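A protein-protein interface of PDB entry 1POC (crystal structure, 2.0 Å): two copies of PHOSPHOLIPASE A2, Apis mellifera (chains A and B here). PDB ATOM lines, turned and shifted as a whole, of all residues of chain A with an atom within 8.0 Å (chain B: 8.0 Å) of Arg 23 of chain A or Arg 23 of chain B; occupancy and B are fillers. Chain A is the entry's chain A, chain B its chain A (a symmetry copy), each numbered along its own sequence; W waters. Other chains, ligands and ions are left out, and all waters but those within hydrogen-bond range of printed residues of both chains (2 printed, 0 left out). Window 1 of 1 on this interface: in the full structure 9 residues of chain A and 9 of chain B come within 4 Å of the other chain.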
ATOM      1  N   TYR A   3      -7.084 -23.583  16.818  1.00  0.00           N
ATOM      2  CA  TYR A   3      -8.340 -23.674  17.577  1.00  0.00           C
ATOM      3  C   TYR A   3      -8.208 -22.870  18.872  1.00  0.00           C
ATOM      4  O   TYR A   3      -7.371 -23.180  19.734  1.00  0.00           O
ATOM      5  CB  TYR A   3      -8.626 -25.148  17.862  1.00  0.00           C
ATOM      6  CG  TYR A   3      -9.874 -25.394  18.708  1.00  0.00           C
ATOM      7  CD1 TYR A   3     -11.144 -25.107  18.194  1.00  0.00           C
ATOM      8  CD2 TYR A   3      -9.741 -25.915  19.997  1.00  0.00           C
ATOM      9  CE1 TYR A   3     -12.283 -25.353  18.970  1.00  0.00           C
ATOM     10  CE2 TYR A   3     -10.877 -26.157  20.774  1.00  0.00           C
ATOM     11  CZ  TYR A   3     -12.148 -25.880  20.259  1.00  0.00           C
ATOM     12  OH  TYR A   3     -13.256 -26.124  21.008  1.00  0.00           O
ATOM     13  N   PRO A   4      -9.012 -21.810  19.059  1.00  0.00           N
ATOM     14  CA  PRO A   4      -8.920 -20.984  20.253  1.00  0.00           C
ATOM     15  C   PRO A   4      -9.096 -21.818  21.496  1.00  0.00           C
ATOM     16  O   PRO A   4     -10.030 -22.675  21.548  1.00  0.00           O
ATOM     17  CB  PRO A   4      -9.984 -19.931  20.046  1.00  0.00           C
ATOM     18  CG  PRO A   4     -10.636 -20.185  18.699  1.00  0.00           C
ATOM     19  CD  PRO A   4     -10.033 -21.409  18.090  1.00  0.00           C
ATOM     20  N   GLY A   5      -8.215 -21.560  22.446  1.00  0.00           N
ATOM     21  CA  GLY A   5      -8.191 -22.273  23.731  1.00  0.00           C
ATOM     22  C   GLY A   5      -7.016 -23.254  23.753  1.00  0.00           C
ATOM     23  O   GLY A   5      -6.756 -23.919  24.766  1.00  0.00           O
ATOM     24  N   THR A   6      -6.354 -23.321  22.616  1.00  0.00           N
ATOM     25  CA  THR A   6      -5.158 -24.153  22.430  1.00  0.00           C
ATOM     26  C   THR A   6      -4.100 -23.315  21.722  1.00  0.00           C
ATOM     27  O   THR A   6      -4.411 -22.301  21.078  1.00  0.00           O
ATOM     28  CB  THR A   6      -5.468 -25.407  21.596  1.00  0.00           C
ATOM     29  OG1 THR A   6      -5.652 -25.056  20.232  1.00  0.00           O
ATOM     30  CG2 THR A   6      -6.728 -26.150  22.055  1.00  0.00           C
ATOM     31  N   LEU A   7      -2.870 -23.745  21.861  1.00  0.00           N
ATOM     32  CA  LEU A   7      -1.743 -23.050  21.244  1.00  0.00           C
ATOM     33  C   LEU A   7      -1.143 -23.883  20.102  1.00  0.00           C
ATOM     34  O   LEU A   7      -0.430 -23.355  19.238  1.00  0.00           O
ATOM     35  CB  LEU A   7      -0.632 -22.799  22.280  1.00  0.00           C
ATOM     36  CG  LEU A   7      -1.001 -21.770  23.357  1.00  0.00           C
ATOM     37  CD1 LEU A   7       0.189 -21.390  24.246  1.00  0.00           C
ATOM     38  CD2 LEU A   7      -1.527 -20.456  22.776  1.00  0.00           C
ATOM     39  N   GLU A  20       4.660 -24.167  26.533  1.00  0.00           N
ATOM     40  CA  GLU A  20       3.397 -23.454  26.795  1.00  0.00           C
ATOM     41  C   GLU A  20       2.205 -24.281  26.296  1.00  0.00           C
ATOM     42  O   GLU A  20       2.258 -24.892  25.219  1.00  0.00           O
ATOM     43  CB  GLU A  20       3.380 -22.105  26.071  1.00  0.00           C
ATOM     44  CG  GLU A  20       3.391 -20.909  27.029  1.00  0.00           C
ATOM     45  CD  GLU A  20       2.285 -19.896  26.734  1.00  0.00           C
ATOM     46  OE1 GLU A  20       2.257 -19.295  25.594  1.00  0.00           O
ATOM     47  OE2 GLU A  20       1.386 -19.645  27.622  1.00  0.00           O
ATOM     48  N   LEU A  21       1.165 -24.272  27.112  1.00  0.00           N
ATOM     49  CA  LEU A  21      -0.117 -24.935  26.811  1.00  0.00           C
ATOM     50  C   LEU A  21      -1.236 -23.909  26.999  1.00  0.00           C
ATOM     51  O   LEU A  21      -1.090 -22.944  27.763  1.00  0.00           O
ATOM     52  CB  LEU A  21      -0.368 -26.112  27.759  1.00  0.00           C
ATOM     53  CG  LEU A  21       0.576 -27.300  27.547  1.00  0.00           C
ATOM     54  CD1 LEU A  21       0.257 -28.477  28.472  1.00  0.00           C
ATOM     55  CD2 LEU A  21       0.530 -27.863  26.124  1.00  0.00           C
ATOM     56  N   GLY A  22      -2.326 -24.145  26.302  1.00  0.00           N
ATOM     57  CA  GLY A  22      -3.487 -23.246  26.326  1.00  0.00           C
ATOM     58  C   GLY A  22      -4.477 -23.639  27.427  1.00  0.00           C
ATOM     59  O   GLY A  22      -4.228 -24.571  28.207  1.00  0.00           O
ATOM     60  N   ARG A  23      -5.559 -22.887  27.416  1.00  0.00           N
ATOM     61  CA  ARG A  23      -6.690 -23.024  28.345  1.00  0.00           C
ATOM     62  C   ARG A  23      -7.122 -24.495  28.461  1.00  0.00           C
ATOM     63  O   ARG A  23      -7.260 -25.038  29.566  1.00  0.00           O
ATOM     64  CB  ARG A  23      -7.839 -22.169  27.816  1.00  0.00           C
ATOM     65  CG  ARG A  23      -9.113 -22.280  28.637  1.00  0.00           C
ATOM     66  CD  ARG A  23     -10.087 -21.135  28.361  1.00  0.00           C
ATOM     67  NE  ARG A  23     -11.469 -21.512  28.658  1.00  0.00           N
ATOM     68  CZ  ARG A  23     -12.507 -21.300  27.845  1.00  0.00           C
ATOM     69  NH1 ARG A  23     -12.353 -20.682  26.664  1.00  0.00           N
ATOM     70  NH2 ARG A  23     -13.753 -21.698  28.127  1.00  0.00           N
ATOM     71  N   PHE A  24      -7.344 -25.114  27.318  1.00  0.00           N
ATOM     72  CA  PHE A  24      -7.703 -26.544  27.252  1.00  0.00           C
ATOM     73  C   PHE A  24      -6.385 -27.325  27.281  1.00  0.00           C
ATOM     74  O   PHE A  24      -5.913 -27.814  26.243  1.00  0.00           O
ATOM     75  CB  PHE A  24      -8.494 -26.811  25.960  1.00  0.00           C
ATOM     76  CG  PHE A  24      -9.791 -25.993  25.876  1.00  0.00           C
ATOM     77  CD1 PHE A  24     -10.668 -25.963  26.966  1.00  0.00           C
ATOM     78  CD2 PHE A  24     -10.102 -25.272  24.713  1.00  0.00           C
ATOM     79  CE1 PHE A  24     -11.849 -25.216  26.898  1.00  0.00           C
ATOM     80  CE2 PHE A  24     -11.285 -24.523  24.645  1.00  0.00           C
ATOM     81  CZ  PHE A  24     -12.158 -24.496  25.738  1.00  0.00           C
ATOM     82  N   LYS A  25      -5.818 -27.417  28.493  1.00  0.00           N
ATOM     83  CA  LYS A  25      -4.462 -27.981  28.678  1.00  0.00           C
ATOM     84  C   LYS A  25      -4.348 -29.474  28.311  1.00  0.00           C
ATOM     85  O   LYS A  25      -3.273 -29.947  27.921  1.00  0.00           O
ATOM     86  CB  LYS A  25      -3.861 -27.708  30.105  1.00  0.00           C
ATOM     87  CG  LYS A  25      -4.665 -28.134  31.351  1.00  0.00           C
ATOM     88  CD  LYS A  25      -3.743 -28.619  32.506  1.00  0.00           C
ATOM     89  CE  LYS A  25      -3.737 -27.710  33.752  1.00  0.00           C
ATOM     90  NZ  LYS A  25      -2.431 -27.681  34.439  1.00  0.00           N
ATOM     91  N   HIS A  26      -5.423 -30.234  28.398  1.00  0.00           N
ATOM     92  CA  HIS A  26      -5.348 -31.680  28.073  1.00  0.00           C
ATOM     93  C   HIS A  26      -5.413 -31.908  26.558  1.00  0.00           C
ATOM     94  O   HIS A  26      -4.679 -32.742  26.006  1.00  0.00           O
ATOM     95  CB  HIS A  26      -6.465 -32.440  28.773  1.00  0.00           C
ATOM     96  CG  HIS A  26      -6.399 -32.244  30.280  1.00  0.00           C
ATOM     97  ND1 HIS A  26      -5.261 -32.574  31.012  1.00  0.00           N
ATOM     98  CD2 HIS A  26      -7.297 -31.754  31.167  1.00  0.00           C
ATOM     99  CE1 HIS A  26      -5.493 -32.281  32.278  1.00  0.00           C
ATOM    100  NE2 HIS A  26      -6.703 -31.791  32.386  1.00  0.00           N
ATOM    101  N   THR A  27      -6.286 -31.163  25.910  1.00  0.00           N
ATOM    102  CA  THR A  27      -6.456 -31.257  24.453  1.00  0.00           C
ATOM    103  C   THR A  27      -5.209 -30.728  23.750  1.00  0.00           C
ATOM    104  O   THR A  27      -4.702 -31.341  22.800  1.00  0.00           O
ATOM    105  CB  THR A  27      -7.658 -30.431  23.992  1.00  0.00           C
ATOM    106  OG1 THR A  27      -8.858 -31.037  24.447  1.00  0.00           O
ATOM    107  CG2 THR A  27      -7.749 -30.309  22.467  1.00  0.00           C
ATOM    108  N   ASP A  28      -4.753 -29.598  24.250  1.00  0.00           N
ATOM    109  CA  ASP A  28      -3.586 -28.903  23.701  1.00  0.00           C
ATOM    110  C   ASP A  28      -2.316 -29.751  23.842  1.00  0.00           C
ATOM    111  O   ASP A  28      -1.445 -29.744  22.962  1.00  0.00           O
ATOM    112  CB  ASP A  28      -3.377 -27.570  24.409  1.00  0.00           C
ATOM    113  CG  ASP A  28      -2.643 -26.571  23.521  1.00  0.00           C
ATOM    114  OD1 ASP A  28      -2.562 -26.786  22.253  1.00  0.00           O
ATOM    115  OD2 ASP A  28      -2.107 -25.522  24.036  1.00  0.00           O
ATOM    116  N   ASP A  76     -10.417 -32.866  28.722  1.00  0.00           N
ATOM    117  CA  ASP A  76     -11.127 -31.766  28.027  1.00  0.00           C
ATOM    118  C   ASP A  76     -11.927 -32.389  26.891  1.00  0.00           C
ATOM    119  O   ASP A  76     -11.600 -32.212  25.711  1.00  0.00           O
ATOM    120  CB  ASP A  76     -10.118 -30.786  27.412  1.00  0.00           C
ATOM    121  CG  ASP A  76      -9.230 -30.083  28.438  1.00  0.00           C
ATOM    122  OD1 ASP A  76      -9.671 -29.862  29.626  1.00  0.00           O
ATOM    123  OD2 ASP A  76      -8.042 -29.708  28.108  1.00  0.00           O
ATOM    124  N   SER A  79     -13.640 -30.153  23.691  1.00  0.00           N
ATOM    125  CA  SER A  79     -12.674 -29.617  22.709  1.00  0.00           C
ATOM    126  C   SER A  79     -11.901 -30.752  22.012  1.00  0.00           C
ATOM    127  O   SER A  79     -11.477 -30.619  20.854  1.00  0.00           O
ATOM    128  CB  SER A  79     -11.696 -28.642  23.379  1.00  0.00           C
ATOM    129  OG  SER A  79     -10.934 -29.297  24.379  1.00  0.00           O
ATOM    130  N   TYR B   3     -19.186 -26.093  16.260  1.00  0.00           N
ATOM    131  CA  TYR B   3     -18.120 -25.427  17.021  1.00  0.00           C
ATOM    132  C   TYR B   3     -18.592 -25.198  18.459  1.00  0.00           C
ATOM    133  O   TYR B   3     -19.567 -24.469  18.702  1.00  0.00           O
ATOM    134  CB  TYR B   3     -17.783 -24.108  16.327  1.00  0.00           C
ATOM    135  CG  TYR B   3     -16.731 -23.269  17.051  1.00  0.00           C
ATOM    136  CD1 TYR B   3     -15.407 -23.716  17.137  1.00  0.00           C
ATOM    137  CD2 TYR B   3     -17.094 -22.045  17.618  1.00  0.00           C
ATOM    138  CE1 TYR B   3     -14.446 -22.932  17.785  1.00  0.00           C
ATOM    139  CE2 TYR B   3     -16.136 -21.264  18.268  1.00  0.00           C
ATOM    140  CZ  TYR B   3     -14.811 -21.705  18.348  1.00  0.00           C
ATOM    141  OH  TYR B   3     -13.874 -20.942  18.971  1.00  0.00           O
ATOM    142  N   PRO B   4     -17.936 -25.809  19.459  1.00  0.00           N
ATOM    143  CA  PRO B   4     -18.349 -25.659  20.846  1.00  0.00           C
ATOM    144  C   PRO B   4     -18.377 -24.205  21.242  1.00  0.00           C
ATOM    145  O   PRO B   4     -17.411 -23.450  20.921  1.00  0.00           O
ATOM    146  CB  PRO B   4     -17.355 -26.501  21.612  1.00  0.00           C
ATOM    147  CG  PRO B   4     -16.410 -27.135  20.608  1.00  0.00           C
ATOM    148  CD  PRO B   4     -16.767 -26.660  19.237  1.00  0.00           C
ATOM    149  N   GLY B   5     -19.461 -23.852  21.911  1.00  0.00           N
ATOM    150  CA  GLY B   5     -19.702 -22.477  22.374  1.00  0.00           C
ATOM    151  C   GLY B   5     -20.771 -21.819  21.497  1.00  0.00           C
ATOM    152  O   GLY B   5     -21.188 -20.679  21.743  1.00  0.00           O
ATOM    153  N   THR B   6     -21.165 -22.565  20.485  1.00  0.00           N
ATOM    154  CA  THR B   6     -22.222 -22.157  19.550  1.00  0.00           C
ATOM    155  C   THR B   6     -23.167 -23.336  19.355  1.00  0.00           C
ATOM    156  O   THR B   6     -22.808 -24.495  19.616  1.00  0.00           O
ATOM    157  CB  THR B   6     -21.638 -21.732  18.192  1.00  0.00           C
ATOM    158  OG1 THR B   6     -21.194 -22.871  17.469  1.00  0.00           O
ATOM    159  CG2 THR B   6     -20.450 -20.771  18.311  1.00  0.00           C
ATOM    160  N   LEU B   7     -24.359 -23.022  18.910  1.00  0.00           N
ATOM    161  CA  LEU B   7     -25.380 -24.040  18.674  1.00  0.00           C
ATOM    162  C   LEU B   7     -25.650 -24.206  17.171  1.00  0.00           C
ATOM    163  O   LEU B   7     -26.201 -25.227  16.735  1.00  0.00           O
ATOM    164  CB  LEU B   7     -26.704 -23.643  19.351  1.00  0.00           C
ATOM    165  CG  LEU B   7     -26.661 -23.684  20.884  1.00  0.00           C
ATOM    166  CD1 LEU B   7     -28.040 -23.487  21.522  1.00  0.00           C
ATOM    167  CD2 LEU B   7     -26.130 -25.011  21.434  1.00  0.00           C
ATOM    168  N   GLU B  20     -32.658 -20.267  20.409  1.00  0.00           N
ATOM    169  CA  GLU B  20     -31.543 -20.530  21.336  1.00  0.00           C
ATOM    170  C   GLU B  20     -30.208 -20.136  20.690  1.00  0.00           C
ATOM    171  O   GLU B  20     -29.979 -20.383  19.498  1.00  0.00           O
ATOM    172  CB  GLU B  20     -31.480 -22.017  21.695  1.00  0.00           C
ATOM    173  CG  GLU B  20     -31.795 -22.293  23.168  1.00  0.00           C
ATOM    174  CD  GLU B  20     -30.737 -23.160  23.854  1.00  0.00           C
ATOM    175  OE1 GLU B  20     -30.513 -24.353  23.424  1.00  0.00           O
ATOM    176  OE2 GLU B  20     -30.073 -22.695  24.856  1.00  0.00           O
ATOM    177  N   LEU B  21     -29.372 -19.525  21.513  1.00  0.00           N
ATOM    178  CA  LEU B  21     -28.006 -19.118  21.137  1.00  0.00           C
ATOM    179  C   LEU B  21     -27.041 -19.678  22.184  1.00  0.00           C
ATOM    180  O   LEU B  21     -27.425 -19.917  23.337  1.00  0.00           O
ATOM    181  CB  LEU B  21     -27.870 -17.592  21.111  1.00  0.00           C
ATOM    182  CG  LEU B  21     -28.646 -16.913  19.978  1.00  0.00           C
ATOM    183  CD1 LEU B  21     -28.439 -15.397  19.950  1.00  0.00           C
ATOM    184  CD2 LEU B  21     -28.250 -17.414  18.587  1.00  0.00           C
ATOM    185  N   GLY B  22     -25.811 -19.866  21.758  1.00  0.00           N
ATOM    186  CA  GLY B  22     -24.759 -20.433  22.613  1.00  0.00           C
ATOM    187  C   GLY B  22     -24.001 -19.338  23.368  1.00  0.00           C
ATOM    188  O   GLY B  22     -24.334 -18.147  23.272  1.00  0.00           O
ATOM    189  N   ARG B  23     -23.006 -19.823  24.083  1.00  0.00           N
ATOM    190  CA  ARG B  23     -22.094 -19.022  24.912  1.00  0.00           C
ATOM    191  C   ARG B  23     -21.579 -17.803  24.129  1.00  0.00           C
ATOM    192  O   ARG B  23     -21.639 -16.661  24.607  1.00  0.00           O
ATOM    193  CB  ARG B  23     -20.932 -19.917  25.333  1.00  0.00           C
ATOM    194  CG  ARG B  23     -19.860 -19.194  26.131  1.00  0.00           C
ATOM    195  CD  ARG B  23     -18.946 -20.157  26.888  1.00  0.00           C
ATOM    196  NE  ARG B  23     -17.634 -19.568  27.155  1.00  0.00           N
ATOM    197  CZ  ARG B  23     -16.465 -20.173  26.925  1.00  0.00           C
ATOM    198  NH1 ARG B  23     -16.412 -21.422  26.439  1.00  0.00           N
ATOM    199  NH2 ARG B  23     -15.282 -19.588  27.139  1.00  0.00           N
ATOM    200  N   PHE B  24     -21.067 -18.065  22.942  1.00  0.00           N
ATOM    201  CA  PHE B  24     -20.587 -17.002  22.038  1.00  0.00           C
ATOM    202  C   PHE B  24     -21.812 -16.501  21.266  1.00  0.00           C
ATOM    203  O   PHE B  24     -22.008 -16.849  20.091  1.00  0.00           O
ATOM    204  CB  PHE B  24     -19.518 -17.580  21.096  1.00  0.00           C
ATOM    205  CG  PHE B  24     -18.304 -18.145  21.848  1.00  0.00           C
ATOM    206  CD1 PHE B  24     -17.688 -17.385  22.848  1.00  0.00           C
ATOM    207  CD2 PHE B  24     -17.809 -19.422  21.541  1.00  0.00           C
ATOM    208  CE1 PHE B  24     -16.584 -17.895  23.540  1.00  0.00           C
ATOM    209  CE2 PHE B  24     -16.705 -19.934  22.235  1.00  0.00           C
ATOM    210  CZ  PHE B  24     -16.093 -19.170  23.234  1.00  0.00           C
ATOM    211  N   LYS B  25     -22.617 -15.688  21.964  1.00  0.00           N
ATOM    212  CA  LYS B  25     -23.931 -15.252  21.439  1.00  0.00           C
ATOM    213  C   LYS B  25     -23.842 -14.376  20.173  1.00  0.00           C
ATOM    214  O   LYS B  25     -24.765 -14.362  19.350  1.00  0.00           O
ATOM    215  CB  LYS B  25     -24.845 -14.575  22.524  1.00  0.00           C
ATOM    216  CG  LYS B  25     -24.296 -13.375  23.324  1.00  0.00           C
ATOM    217  CD  LYS B  25     -25.402 -12.331  23.648  1.00  0.00           C
ATOM    218  CE  LYS B  25     -25.750 -12.203  25.145  1.00  0.00           C
ATOM    219  NZ  LYS B  25     -27.171 -11.882  25.383  1.00  0.00           N
ATOM    220  N   HIS B  26     -22.753 -13.660  19.972  1.00  0.00           N
ATOM    221  CA  HIS B  26     -22.638 -12.789  18.776  1.00  0.00           C
ATOM    222  C   HIS B  26     -22.230 -13.600  17.540  1.00  0.00           C
ATOM    223  O   HIS B  26     -22.758 -13.393  16.437  1.00  0.00           O
ATOM    224  CB  HIS B  26     -21.640 -11.669  19.027  1.00  0.00           C
ATOM    225  CG  HIS B  26     -22.044 -10.838  20.236  1.00  0.00           C
ATOM    226  ND1 HIS B  26     -23.281 -10.204  20.307  1.00  0.00           N
ATOM    227  CD2 HIS B  26     -21.400 -10.555  21.394  1.00  0.00           C
ATOM    228  CE1 HIS B  26     -23.352  -9.580  21.468  1.00  0.00           C
ATOM    229  NE2 HIS B  26     -22.238  -9.779  22.127  1.00  0.00           N
ATOM    230  N   THR B  27     -21.302 -14.514  17.744  1.00  0.00           N
ATOM    231  CA  THR B  27     -20.816 -15.380  16.660  1.00  0.00           C
ATOM    232  C   THR B  27     -21.921 -16.339  16.227  1.00  0.00           C
ATOM    233  O   THR B  27     -22.160 -16.539  15.027  1.00  0.00           O
ATOM    234  CB  THR B  27     -19.613 -16.206  17.124  1.00  0.00           C
ATOM    235  OG1 THR B  27     -18.494 -15.355  17.316  1.00  0.00           O
ATOM    236  CG2 THR B  27     -19.207 -17.286  16.115  1.00  0.00           C
ATOM    237  N   ASP B  28     -22.564 -16.901  17.230  1.00  0.00           N
ATOM    238  CA  ASP B  28     -23.638 -17.877  17.034  1.00  0.00           C
ATOM    239  C   ASP B  28     -24.835 -17.250  16.310  1.00  0.00           C
ATOM    240  O   ASP B  28     -25.495 -17.901  15.487  1.00  0.00           O
ATOM    241  CB  ASP B  28     -24.103 -18.437  18.374  1.00  0.00           C
ATOM    242  CG  ASP B  28     -24.707 -19.828  18.223  1.00  0.00           C
ATOM    243  OD1 ASP B  28     -24.496 -20.501  17.143  1.00  0.00           O
ATOM    244  OD2 ASP B  28     -25.424 -20.325  19.166  1.00  0.00           O
ATOM    245  N   ASP B  76     -17.748 -11.060  19.563  1.00  0.00           N
ATOM    246  CA  ASP B  76     -16.997 -12.284  19.929  1.00  0.00           C
ATOM    247  C   ASP B  76     -15.923 -12.492  18.869  1.00  0.00           C
ATOM    248  O   ASP B  76     -16.002 -13.422  18.057  1.00  0.00           O
ATOM    249  CB  ASP B  76     -17.927 -13.506  19.905  1.00  0.00           C
ATOM    250  CG  ASP B  76     -19.068 -13.438  20.917  1.00  0.00           C
ATOM    251  OD1 ASP B  76     -18.913 -12.793  22.020  1.00  0.00           O
ATOM    252  OD2 ASP B  76     -20.184 -14.032  20.667  1.00  0.00           O
ATOM    253  N   SER B  79     -13.750 -16.126  18.373  1.00  0.00           N
ATOM    254  CA  SER B  79     -14.522 -17.249  17.802  1.00  0.00           C
ATOM    255  C   SER B  79     -15.033 -16.912  16.388  1.00  0.00           C
ATOM    256  O   SER B  79     -15.207 -17.802  15.542  1.00  0.00           O
ATOM    257  CB  SER B  79     -15.697 -17.625  18.715  1.00  0.00           C
ATOM    258  OG  SER B  79     -16.601 -16.541  18.850  1.00  0.00           O
HETATM  259  O   HOH W   1     -12.741 -21.964  21.458  1.00  0.00           O
HETATM  260  O   HOH W   2     -14.810 -23.824  21.903  1.00  0.00           O
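Water W1 lies within hydrogen-bond range of the backbone carbonyl oxygen of Pro 4 of chain A (2.8 Å) and the side-chain hydroxyl of Tyr 3 of chain B (2.9 Å).
Water W2 bridges O of Pro 4 of chain B and OH of Tyr 3 of chain A.
Tyr 3 of chain A touches its own counterpart, Tyr 3 of chain B.
Tyr 3 of chain A touches Pro 4 of chain B, and with the chains exchanged Pro 4 of chain A touches Tyr 3 of chain B.
Arg 23 of chain B touches its own counterpart, Arg 23 of chain A.
The guanidinium group (NH2) of Arg 23 of chain A lies close to the guanidinium group (NH2) of Arg 23 of chain B, at 2.8 Å.
Among the printed residues, merely in contact across the chains: Tyr 3 of chain A with Tyr 3 of chain B (3.5 Å), Tyr 3 of chain A with Pro 4 of chain B (3.3 Å) and Pro 4 of chain A with Tyr 3 of chain B (3.3 Å).
Of the 16 printed residues of chain B, 3 touch a printed residue of chain A.
Printed residues of chain B that touch a printed residue of chain A: Tyr 3, Pro 4 and Arg 23.
Along chain B the printed residues that touch a printed residue of chain A span positions 3 to 23.
Of the printed residues of chain B, Pro 4 of chain A touches Tyr 3.
Thr 6 of chain A touches none of the printed residues of chain B.
No residue of chain B comes within 4 Å of Gly 22 of chain A.
Arg 23 of chain A touches just one residue of chain B: Arg 23 (2.8 Å).
Printed residues of chain A within 4 Å of Tyr 3 of chain B: Tyr 3 and Pro 4.
Of the printed residues of chain A, Pro 4 of chain B touches Tyr 3.
Thr 6 of chain B touches none of the printed residues of chain A.
Gly 22 of chain B touches none of the printed residues of chain A.
Of chain A, only Arg 23 comes within 4 Å of Arg 23 of chain B.
The nearest printed residue of chain B that does not touch Pro 4 of chain A is Ser 79 of chain B (5.0 Å).
The backbone carbonyl oxygen of Tyr 3 of chain A sits at hydrogen-bond distance from the side-chain hydroxyl of Thr 6 of chain A, at 2.6 Å.
O of Gly 5 of chain A sits at hydrogen-bond distance from N of Arg 23 of chain A (3.1 Å).
The backbone carbonyl oxygen (O) of Tyr 3 of chain B is in hydrogen-bond range of the side-chain hydroxyl (OG1) of Thr 6 of chain B (2.6 Å).
The backbone carbonyl oxygen (O) of Gly 5 of chain B lies within hydrogen-bond range of the backbone NH (N) of Arg 23 of chain B (3.1 Å).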
